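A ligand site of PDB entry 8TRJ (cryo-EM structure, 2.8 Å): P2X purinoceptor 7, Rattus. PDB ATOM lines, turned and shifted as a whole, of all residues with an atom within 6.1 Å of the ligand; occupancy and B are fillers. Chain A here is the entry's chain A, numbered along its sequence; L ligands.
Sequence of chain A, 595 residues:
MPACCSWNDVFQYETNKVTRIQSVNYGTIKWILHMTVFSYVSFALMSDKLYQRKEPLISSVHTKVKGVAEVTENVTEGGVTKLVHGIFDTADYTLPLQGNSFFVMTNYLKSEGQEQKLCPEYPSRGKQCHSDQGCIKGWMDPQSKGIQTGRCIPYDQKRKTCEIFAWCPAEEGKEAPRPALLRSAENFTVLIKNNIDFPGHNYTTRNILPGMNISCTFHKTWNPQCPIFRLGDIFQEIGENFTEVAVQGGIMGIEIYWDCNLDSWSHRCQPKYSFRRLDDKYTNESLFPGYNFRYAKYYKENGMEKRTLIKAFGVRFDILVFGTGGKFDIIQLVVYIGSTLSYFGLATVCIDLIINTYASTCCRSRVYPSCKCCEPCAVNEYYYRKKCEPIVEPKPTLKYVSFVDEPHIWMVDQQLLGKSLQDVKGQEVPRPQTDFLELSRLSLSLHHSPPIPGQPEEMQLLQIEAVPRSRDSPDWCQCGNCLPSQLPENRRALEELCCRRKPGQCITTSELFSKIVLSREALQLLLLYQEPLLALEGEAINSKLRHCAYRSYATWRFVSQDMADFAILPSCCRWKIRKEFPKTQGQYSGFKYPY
Merely in contact with the ligand: Ala 564 (3.6 Å), Asp 565 (3.6 Å), Phe 591 (3.7 Å), Tyr 588 (3.7 Å), Lys 592 (3.7 Å), Gly 590 (3.7 Å) and Ile 568 (3.8 Å).
16 residues have an atom within 4 Å of the ligand: Arg 546, His 547, Tyr 550, Ala 564, Asp 565, Ala 567, Ile 568, Leu 569, Arg 574, Arg 578, Lys 583, Tyr 588, Ser 589, Gly 590, Phe 591 and Lys 592.
The guanidinium group of Arg 574 lies within hydrogen-bond range of the backbone carbonyl oxygen of Leu 569, 3.3 Å away.
OH of Tyr 588 lies close to N of Lys 583 (3.4 Å).
NZ of Lys 583 sits at hydrogen-bond distance from O of Gln 587 (2.8 Å).
NE2 of His 547 lies close to O of Ser 543 (3.3 Å).
O of Ser 589 is in hydrogen-bond range of NH2 of Arg 578.
NE of Arg 578 is in hydrogen-bond range of OH of Tyr 550 (2.4 Å).
The guanidinium group of Arg 574 is in hydrogen-bond range of an oxygen (O11) of the ligand (2.5 Å).
The guanidinium group (NH1) of Arg 546 is in salt-bridge range of an oxygen (O5) of the ligand.
The side-chain amino group (NZ) of Lys 583 is in salt-bridge range of an oxygen (O2) of the ligand (2.9 Å).
A nitrogen (N4) of the ligand sits at hydrogen-bond distance from the backbone carbonyl oxygen of Ala 567, at 2.9 Å.
O11 of the ligand lies within hydrogen-bond range of N of Leu 569, 2.9 Å away.
NE2 of His 547 is in hydrogen-bond range of O5 of the ligand (2.9 Å).
An oxygen (O2) of the ligand sits at hydrogen-bond distance from the backbone NH of Ser 589.
NH2 of Arg 578 is in salt-bridge range of O6 of the ligand (3.2 Å).
The side-chain hydroxyl (OH) of Tyr 550 sits close to an oxygen (O6) of the ligand (3.4 Å).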
ATOM      1  N   LEU A 494       7.473  17.113   9.422  1.00  0.00           N
ATOM      2  CA  LEU A 494       8.500  17.973   8.848  1.00  0.00           C
ATOM      3  C   LEU A 494       7.898  19.215   8.212  1.00  0.00           C
ATOM      4  O   LEU A 494       8.411  20.322   8.410  1.00  0.00           O
ATOM      5  CB  LEU A 494       9.316  17.169   7.837  1.00  0.00           C
ATOM      6  CG  LEU A 494      10.477  17.875   7.135  1.00  0.00           C
ATOM      7  CD1 LEU A 494      11.545  16.851   6.788  1.00  0.00           C
ATOM      8  CD2 LEU A 494      10.000  18.580   5.867  1.00  0.00           C
ATOM      9  N   GLU A 495       6.823  19.051   7.451  1.00  0.00           N
ATOM     10  CA  GLU A 495       6.236  20.165   6.701  1.00  0.00           C
ATOM     11  C   GLU A 495       5.401  21.091   7.564  1.00  0.00           C
ATOM     12  O   GLU A 495       4.909  22.100   7.054  1.00  0.00           O
ATOM     13  CB  GLU A 495       5.391  19.626   5.551  1.00  0.00           C
ATOM     14  CG  GLU A 495       6.193  19.014   4.418  1.00  0.00           C
ATOM     15  CD  GLU A 495       5.347  18.731   3.194  1.00  0.00           C
ATOM     16  OE1 GLU A 495       4.117  18.968   3.248  1.00  0.00           O
ATOM     17  OE2 GLU A 495       5.895  18.263   2.185  1.00  0.00           O
ATOM     18  N   SER A 543       7.517  21.594 -12.812  1.00  0.00           N
ATOM     19  CA  SER A 543       8.191  20.950 -11.694  1.00  0.00           C
ATOM     20  C   SER A 543       9.589  21.510 -11.513  1.00  0.00           C
ATOM     21  O   SER A 543       9.990  21.892 -10.409  1.00  0.00           O
ATOM     22  CB  SER A 543       8.247  19.442 -11.899  1.00  0.00           C
ATOM     23  OG  SER A 543       9.142  19.101 -12.939  1.00  0.00           O
ATOM     24  N   ARG A 546       9.455  24.776  -9.908  1.00  0.00           N
ATOM     25  CA  ARG A 546       9.208  24.615  -8.489  1.00  0.00           C
ATOM     26  C   ARG A 546      10.495  24.337  -7.741  1.00  0.00           C
ATOM     27  O   ARG A 546      10.811  25.002  -6.747  1.00  0.00           O
ATOM     28  CB  ARG A 546       8.199  23.485  -8.262  1.00  0.00           C
ATOM     29  CG  ARG A 546       7.167  23.788  -7.211  1.00  0.00           C
ATOM     30  CD  ARG A 546       6.269  22.598  -6.959  1.00  0.00           C
ATOM     31  NE  ARG A 546       5.745  22.039  -8.197  1.00  0.00           N
ATOM     32  CZ  ARG A 546       6.045  20.848  -8.691  1.00  0.00           C
ATOM     33  NH1 ARG A 546       6.880  20.031  -8.058  1.00  0.00           N
ATOM     34  NH2 ARG A 546       5.506  20.452  -9.839  1.00  0.00           N
ATOM     35  N   HIS A 547      11.285  23.389  -8.245  1.00  0.00           N
ATOM     36  CA  HIS A 547      12.553  23.082  -7.582  1.00  0.00           C
ATOM     37  C   HIS A 547      13.412  24.334  -7.493  1.00  0.00           C
ATOM     38  O   HIS A 547      13.970  24.648  -6.437  1.00  0.00           O
ATOM     39  CB  HIS A 547      13.288  21.973  -8.336  1.00  0.00           C
ATOM     40  CG  HIS A 547      12.446  20.783  -8.645  1.00  0.00           C
ATOM     41  ND1 HIS A 547      12.844  19.805  -9.536  1.00  0.00           N
ATOM     42  CD2 HIS A 547      11.233  20.403  -8.193  1.00  0.00           C
ATOM     43  CE1 HIS A 547      11.914  18.874  -9.613  1.00  0.00           C
ATOM     44  NE2 HIS A 547      10.918  19.220  -8.808  1.00  0.00           N
ATOM     45  N   TYR A 550      12.311  26.451  -4.717  1.00  0.00           N
ATOM     46  CA  TYR A 550      12.763  25.907  -3.446  1.00  0.00           C
ATOM     47  C   TYR A 550      14.197  26.306  -3.180  1.00  0.00           C
ATOM     48  O   TYR A 550      14.545  26.741  -2.069  1.00  0.00           O
ATOM     49  CB  TYR A 550      12.635  24.381  -3.433  1.00  0.00           C
ATOM     50  CG  TYR A 550      11.214  23.873  -3.549  1.00  0.00           C
ATOM     51  CD1 TYR A 550      10.154  24.610  -3.050  1.00  0.00           C
ATOM     52  CD2 TYR A 550      10.941  22.661  -4.151  1.00  0.00           C
ATOM     53  CE1 TYR A 550       8.864  24.149  -3.159  1.00  0.00           C
ATOM     54  CE2 TYR A 550       9.665  22.199  -4.260  1.00  0.00           C
ATOM     55  CZ  TYR A 550       8.627  22.947  -3.761  1.00  0.00           C
ATOM     56  OH  TYR A 550       7.338  22.493  -3.863  1.00  0.00           O
ATOM     57  N   ALA A 554      15.597  28.829  -0.234  1.00  0.00           N
ATOM     58  CA  ALA A 554      16.607  28.264   0.639  1.00  0.00           C
ATOM     59  C   ALA A 554      17.879  29.077   0.599  1.00  0.00           C
ATOM     60  O   ALA A 554      18.647  29.087   1.565  1.00  0.00           O
ATOM     61  CB  ALA A 554      16.887  26.819   0.248  1.00  0.00           C
ATOM     62  N   ALA A 564      21.460  25.157   2.883  1.00  0.00           N
ATOM     63  CA  ALA A 564      20.255  25.316   2.078  1.00  0.00           C
ATOM     64  C   ALA A 564      19.769  24.020   1.443  1.00  0.00           C
ATOM     65  O   ALA A 564      18.594  23.934   1.085  1.00  0.00           O
ATOM     66  CB  ALA A 564      20.509  26.358   0.984  1.00  0.00           C
ATOM     67  N   ASP A 565      20.648  23.020   1.285  1.00  0.00           N
ATOM     68  CA  ASP A 565      20.176  21.713   0.841  1.00  0.00           C
ATOM     69  C   ASP A 565      19.224  21.092   1.860  1.00  0.00           C
ATOM     70  O   ASP A 565      18.212  20.485   1.493  1.00  0.00           O
ATOM     71  CB  ASP A 565      21.337  20.766   0.564  1.00  0.00           C
ATOM     72  CG  ASP A 565      22.349  21.308  -0.420  1.00  0.00           C
ATOM     73  OD1 ASP A 565      23.144  22.180  -0.038  1.00  0.00           O
ATOM     74  OD2 ASP A 565      22.372  20.832  -1.571  1.00  0.00           O
ATOM     75  N   PHE A 566      19.544  21.228   3.141  1.00  0.00           N
ATOM     76  CA  PHE A 566      18.791  20.588   4.204  1.00  0.00           C
ATOM     77  C   PHE A 566      17.747  21.499   4.822  1.00  0.00           C
ATOM     78  O   PHE A 566      17.054  21.088   5.760  1.00  0.00           O
ATOM     79  CB  PHE A 566      19.729  20.093   5.291  1.00  0.00           C
ATOM     80  CG  PHE A 566      20.506  18.869   4.900  1.00  0.00           C
ATOM     81  CD1 PHE A 566      19.961  17.603   5.062  1.00  0.00           C
ATOM     82  CD2 PHE A 566      21.762  18.981   4.352  1.00  0.00           C
ATOM     83  CE1 PHE A 566      20.668  16.491   4.704  1.00  0.00           C
ATOM     84  CE2 PHE A 566      22.469  17.869   3.994  1.00  0.00           C
ATOM     85  CZ  PHE A 566      21.918  16.622   4.164  1.00  0.00           C
ATOM     86  N   ALA A 567      17.610  22.722   4.321  1.00  0.00           N
ATOM     87  CA  ALA A 567      16.582  23.617   4.820  1.00  0.00           C
ATOM     88  C   ALA A 567      15.202  23.063   4.540  1.00  0.00           C
ATOM     89  O   ALA A 567      15.005  22.192   3.685  1.00  0.00           O
ATOM     90  CB  ALA A 567      16.726  24.988   4.182  1.00  0.00           C
ATOM     91  N   ILE A 568      14.213  23.566   5.276  1.00  0.00           N
ATOM     92  CA  ILE A 568      12.828  23.183   5.121  1.00  0.00           C
ATOM     93  C   ILE A 568      12.023  24.445   4.889  1.00  0.00           C
ATOM     94  O   ILE A 568      12.101  25.393   5.686  1.00  0.00           O
ATOM     95  CB  ILE A 568      12.306  22.405   6.341  1.00  0.00           C
ATOM     96  CG1 ILE A 568      13.294  21.332   6.776  1.00  0.00           C
ATOM     97  CG2 ILE A 568      10.967  21.767   6.015  1.00  0.00           C
ATOM     98  CD1 ILE A 568      13.553  20.265   5.745  1.00  0.00           C
ATOM     99  N   LEU A 569      11.266  24.464   3.815  1.00  0.00           N
ATOM    100  CA  LEU A 569      10.429  25.610   3.506  1.00  0.00           C
ATOM    101  C   LEU A 569       9.173  25.620   4.384  1.00  0.00           C
ATOM    102  O   LEU A 569       8.626  24.562   4.704  1.00  0.00           O
ATOM    103  CB  LEU A 569      10.017  25.587   2.050  1.00  0.00           C
ATOM    104  CG  LEU A 569      10.933  26.291   1.048  1.00  0.00           C
ATOM    105  CD1 LEU A 569      12.215  25.529   0.836  1.00  0.00           C
ATOM    106  CD2 LEU A 569      10.185  26.455  -0.248  1.00  0.00           C
ATOM    107  N   PRO A 570       8.698  26.793   4.783  1.00  0.00           N
ATOM    108  CA  PRO A 570       7.418  26.862   5.493  1.00  0.00           C
ATOM    109  C   PRO A 570       6.265  26.456   4.590  1.00  0.00           C
ATOM    110  O   PRO A 570       6.361  26.478   3.356  1.00  0.00           O
ATOM    111  CB  PRO A 570       7.318  28.329   5.898  1.00  0.00           C
ATOM    112  CG  PRO A 570       8.690  28.844   5.848  1.00  0.00           C
ATOM    113  CD  PRO A 570       9.365  28.101   4.756  1.00  0.00           C
ATOM    114  N   ARG A 574       5.754  27.204   0.524  1.00  0.00           N
ATOM    115  CA  ARG A 574       5.692  25.999  -0.305  1.00  0.00           C
ATOM    116  C   ARG A 574       4.395  25.936  -1.093  1.00  0.00           C
ATOM    117  O   ARG A 574       4.392  25.618  -2.283  1.00  0.00           O
ATOM    118  CB  ARG A 574       5.843  24.763   0.584  1.00  0.00           C
ATOM    119  CG  ARG A 574       5.905  23.460  -0.179  1.00  0.00           C
ATOM    120  CD  ARG A 574       5.664  22.272   0.746  1.00  0.00           C
ATOM    121  NE  ARG A 574       6.587  22.273   1.869  1.00  0.00           N
ATOM    122  CZ  ARG A 574       7.824  21.817   1.818  1.00  0.00           C
ATOM    123  NH1 ARG A 574       8.308  21.319   0.685  1.00  0.00           N
ATOM    124  NH2 ARG A 574       8.591  21.851   2.892  1.00  0.00           N
ATOM    125  N   ARG A 578       3.599  26.061  -5.050  1.00  0.00           N
ATOM    126  CA  ARG A 578       2.831  25.029  -5.738  1.00  0.00           C
ATOM    127  C   ARG A 578       1.684  25.627  -6.527  1.00  0.00           C
ATOM    128  O   ARG A 578       1.400  25.203  -7.657  1.00  0.00           O
ATOM    129  CB  ARG A 578       2.305  24.001  -4.733  1.00  0.00           C
ATOM    130  CG  ARG A 578       3.165  22.762  -4.594  1.00  0.00           C
ATOM    131  CD  ARG A 578       4.240  22.977  -3.559  1.00  0.00           C
ATOM    132  NE  ARG A 578       5.063  21.783  -3.361  1.00  0.00           N
ATOM    133  CZ  ARG A 578       4.908  20.907  -2.373  1.00  0.00           C
ATOM    134  NH1 ARG A 578       3.960  21.056  -1.459  1.00  0.00           N
ATOM    135  NH2 ARG A 578       5.723  19.867  -2.284  1.00  0.00           N
ATOM    136  N   LYS A 583       1.002  20.906 -10.095  1.00  0.00           N
ATOM    137  CA  LYS A 583       1.311  19.619 -10.724  1.00  0.00           C
ATOM    138  C   LYS A 583       0.035  18.791 -10.772  1.00  0.00           C
ATOM    139  O   LYS A 583      -0.395  18.229  -9.756  1.00  0.00           O
ATOM    140  CB  LYS A 583       2.414  18.899  -9.960  1.00  0.00           C
ATOM    141  CG  LYS A 583       2.813  17.556 -10.551  1.00  0.00           C
ATOM    142  CD  LYS A 583       3.721  16.788  -9.606  1.00  0.00           C
ATOM    143  CE  LYS A 583       2.954  16.207  -8.442  1.00  0.00           C
ATOM    144  NZ  LYS A 583       3.830  15.413  -7.540  1.00  0.00           N
ATOM    145  N   GLN A 587      -0.234  14.143  -6.113  1.00  0.00           N
ATOM    146  CA  GLN A 587       0.106  14.809  -4.869  1.00  0.00           C
ATOM    147  C   GLN A 587       1.566  15.235  -4.874  1.00  0.00           C
ATOM    148  O   GLN A 587       2.443  14.477  -5.300  1.00  0.00           O
ATOM    149  CB  GLN A 587      -0.179  13.891  -3.684  1.00  0.00           C
ATOM    150  N   TYR A 588       1.835  16.444  -4.389  1.00  0.00           N
ATOM    151  CA  TYR A 588       3.196  16.948  -4.335  1.00  0.00           C
ATOM    152  C   TYR A 588       4.002  16.196  -3.292  1.00  0.00           C
ATOM    153  O   TYR A 588       3.509  15.924  -2.187  1.00  0.00           O
ATOM    154  CB  TYR A 588       3.208  18.452  -4.028  1.00  0.00           C
ATOM    155  CG  TYR A 588       2.245  19.271  -4.843  1.00  0.00           C
ATOM    156  CD1 TYR A 588       2.521  19.608  -6.161  1.00  0.00           C
ATOM    157  CD2 TYR A 588       1.056  19.738  -4.286  1.00  0.00           C
ATOM    158  CE1 TYR A 588       1.649  20.366  -6.905  1.00  0.00           C
ATOM    159  CE2 TYR A 588       0.185  20.504  -5.023  1.00  0.00           C
ATOM    160  CZ  TYR A 588       0.473  20.807  -6.333  1.00  0.00           C
ATOM    161  OH  TYR A 588      -0.405  21.568  -7.065  1.00  0.00           O
ATOM    162  N   SER A 589       5.245  15.876  -3.630  1.00  0.00           N
ATOM    163  CA  SER A 589       6.153  15.237  -2.693  1.00  0.00           C
ATOM    164  C   SER A 589       6.714  16.307  -1.756  1.00  0.00           C
ATOM    165  O   SER A 589       6.238  17.448  -1.710  1.00  0.00           O
ATOM    166  CB  SER A 589       7.245  14.484  -3.433  1.00  0.00           C
ATOM    167  OG  SER A 589       7.875  13.537  -2.588  1.00  0.00           O
ATOM    168  N   GLY A 590       7.741  15.947  -0.993  1.00  0.00           N
ATOM    169  CA  GLY A 590       8.321  16.873  -0.033  1.00  0.00           C
ATOM    170  C   GLY A 590       9.829  16.806   0.023  1.00  0.00           C
ATOM    171  O   GLY A 590      10.476  16.297  -0.907  1.00  0.00           O
ATOM    172  N   PHE A 591      10.414  17.314   1.102  1.00  0.00           N
ATOM    173  CA  PHE A 591      11.860  17.342   1.224  1.00  0.00           C
ATOM    174  C   PHE A 591      12.438  15.941   1.126  1.00  0.00           C
ATOM    175  O   PHE A 591      11.978  15.019   1.809  1.00  0.00           O
ATOM    176  CB  PHE A 591      12.273  17.996   2.534  1.00  0.00           C
ATOM    177  CG  PHE A 591      13.739  17.900   2.821  1.00  0.00           C
ATOM    178  CD1 PHE A 591      14.666  18.478   1.972  1.00  0.00           C
ATOM    179  CD2 PHE A 591      14.205  17.225   3.936  1.00  0.00           C
ATOM    180  CE1 PHE A 591      16.011  18.390   2.235  1.00  0.00           C
ATOM    181  CE2 PHE A 591      15.549  17.129   4.192  1.00  0.00           C
ATOM    182  CZ  PHE A 591      16.455  17.714   3.339  1.00  0.00           C
ATOM    183  N   LYS A 592      13.445  15.780   0.279  1.00  0.00           N
ATOM    184  CA  LYS A 592      14.134  14.517   0.090  1.00  0.00           C
ATOM    185  C   LYS A 592      15.613  14.710   0.399  1.00  0.00           C
ATOM    186  O   LYS A 592      16.148  15.820   0.248  1.00  0.00           O
ATOM    187  CB  LYS A 592      13.960  13.996  -1.334  1.00  0.00           C
ATOM    188  CG  LYS A 592      14.585  12.637  -1.574  1.00  0.00           C
ATOM    189  CD  LYS A 592      14.077  12.029  -2.865  1.00  0.00           C
ATOM    190  CE  LYS A 592      14.456  12.885  -4.065  1.00  0.00           C
ATOM    191  NZ  LYS A 592      14.803  12.063  -5.244  1.00  0.00           N
ATOM    192  N   TYR A 593      16.260  13.638   0.827  1.00  0.00           N
ATOM    193  CA  TYR A 593      17.645  13.738   1.251  1.00  0.00           C
ATOM    194  C   TYR A 593      18.502  14.282   0.103  1.00  0.00           C
ATOM    195  O   TYR A 593      18.432  13.771  -1.015  1.00  0.00           O
ATOM    196  CB  TYR A 593      18.160  12.370   1.676  1.00  0.00           C
ATOM    197  CG  TYR A 593      19.553  12.396   2.271  1.00  0.00           C
ATOM    198  CD1 TYR A 593      19.806  13.067   3.460  1.00  0.00           C
ATOM    199  CD2 TYR A 593      20.607  11.761   1.645  1.00  0.00           C
ATOM    200  CE1 TYR A 593      21.063  13.096   4.007  1.00  0.00           C
ATOM    201  CE2 TYR A 593      21.878  11.791   2.174  1.00  0.00           C
ATOM    202  CZ  TYR A 593      22.095  12.461   3.353  1.00  0.00           C
ATOM    203  OH  TYR A 593      23.358  12.487   3.888  1.00  0.00           O
ATOM    204  N   PRO A 594      19.310  15.322   0.342  1.00  0.00           N
ATOM    205  CA  PRO A 594      20.113  15.881  -0.756  1.00  0.00           C
ATOM    206  C   PRO A 594      21.035  14.867  -1.411  1.00  0.00           C
ATOM    207  O   PRO A 594      21.196  14.905  -2.639  1.00  0.00           O
ATOM    208  CB  PRO A 594      20.901  16.991  -0.054  1.00  0.00           C
ATOM    209  CG  PRO A 594      20.055  17.384   1.072  1.00  0.00           C
ATOM    210  CD  PRO A 594      19.453  16.132   1.569  1.00  0.00           C
HETATM  211  P1  LIG L   1       7.097  16.560  -6.601  1.00  0.00           P
HETATM  212  O1  LIG L   1       6.040  17.637  -6.614  1.00  0.00           O
HETATM  213  O2  LIG L   1       6.450  15.212  -6.382  1.00  0.00           O
HETATM  214  O3  LIG L   1       7.849  16.565  -7.903  1.00  0.00           O
HETATM  215  O4  LIG L   1       8.128  16.857  -5.398  1.00  0.00           O
HETATM  216  P2  LIG L   1       8.849  18.281  -5.320  1.00  0.00           P
HETATM  217  O5  LIG L   1       8.963  18.887  -6.694  1.00  0.00           O
HETATM  218  O6  LIG L   1       8.094  19.205  -4.390  1.00  0.00           O
HETATM  219  O7  LIG L   1      10.303  17.929  -4.703  1.00  0.00           O
HETATM  220  C1  LIG L   1      11.423  17.787  -5.568  1.00  0.00           C
HETATM  221  C2  LIG L   1      12.657  18.369  -4.914  1.00  0.00           C
HETATM  222  O8  LIG L   1      12.286  19.534  -4.188  1.00  0.00           O
HETATM  223  C3  LIG L   1      13.311  17.401  -3.944  1.00  0.00           C
HETATM  224  O9  LIG L   1      14.541  16.905  -4.489  1.00  0.00           O
HETATM  225  C4  LIG L   1      13.554  18.201  -2.687  1.00  0.00           C
HETATM  226  O10 LIG L   1      14.938  18.222  -2.325  1.00  0.00           O
HETATM  227  C5  LIG L   1      13.053  19.598  -2.982  1.00  0.00           C
HETATM  228  N1  LIG L   1      12.222  20.111  -1.871  1.00  0.00           N
HETATM  229  C6  LIG L   1      10.905  19.933  -1.707  1.00  0.00           C
HETATM  230  N2  LIG L   1      10.479  20.564  -0.577  1.00  0.00           N
HETATM  231  C7  LIG L   1      11.546  21.147  -0.010  1.00  0.00           C
HETATM  232  C8  LIG L   1      11.816  21.961   1.184  1.00  0.00           C
HETATM  233  O11 LIG L   1      10.894  22.258   1.975  1.00  0.00           O
HETATM  234  N3  LIG L   1      13.065  22.378   1.405  1.00  0.00           N
HETATM  235  C9  LIG L   1      14.068  22.064   0.563  1.00  0.00           C
HETATM  236  N4  LIG L   1      15.321  22.517   0.835  1.00  0.00           N
HETATM  237  N5  LIG L   1      13.899  21.329  -0.549  1.00  0.00           N
HETATM  238  C10 LIG L   1      12.685  20.856  -0.877  1.00  0.00           C
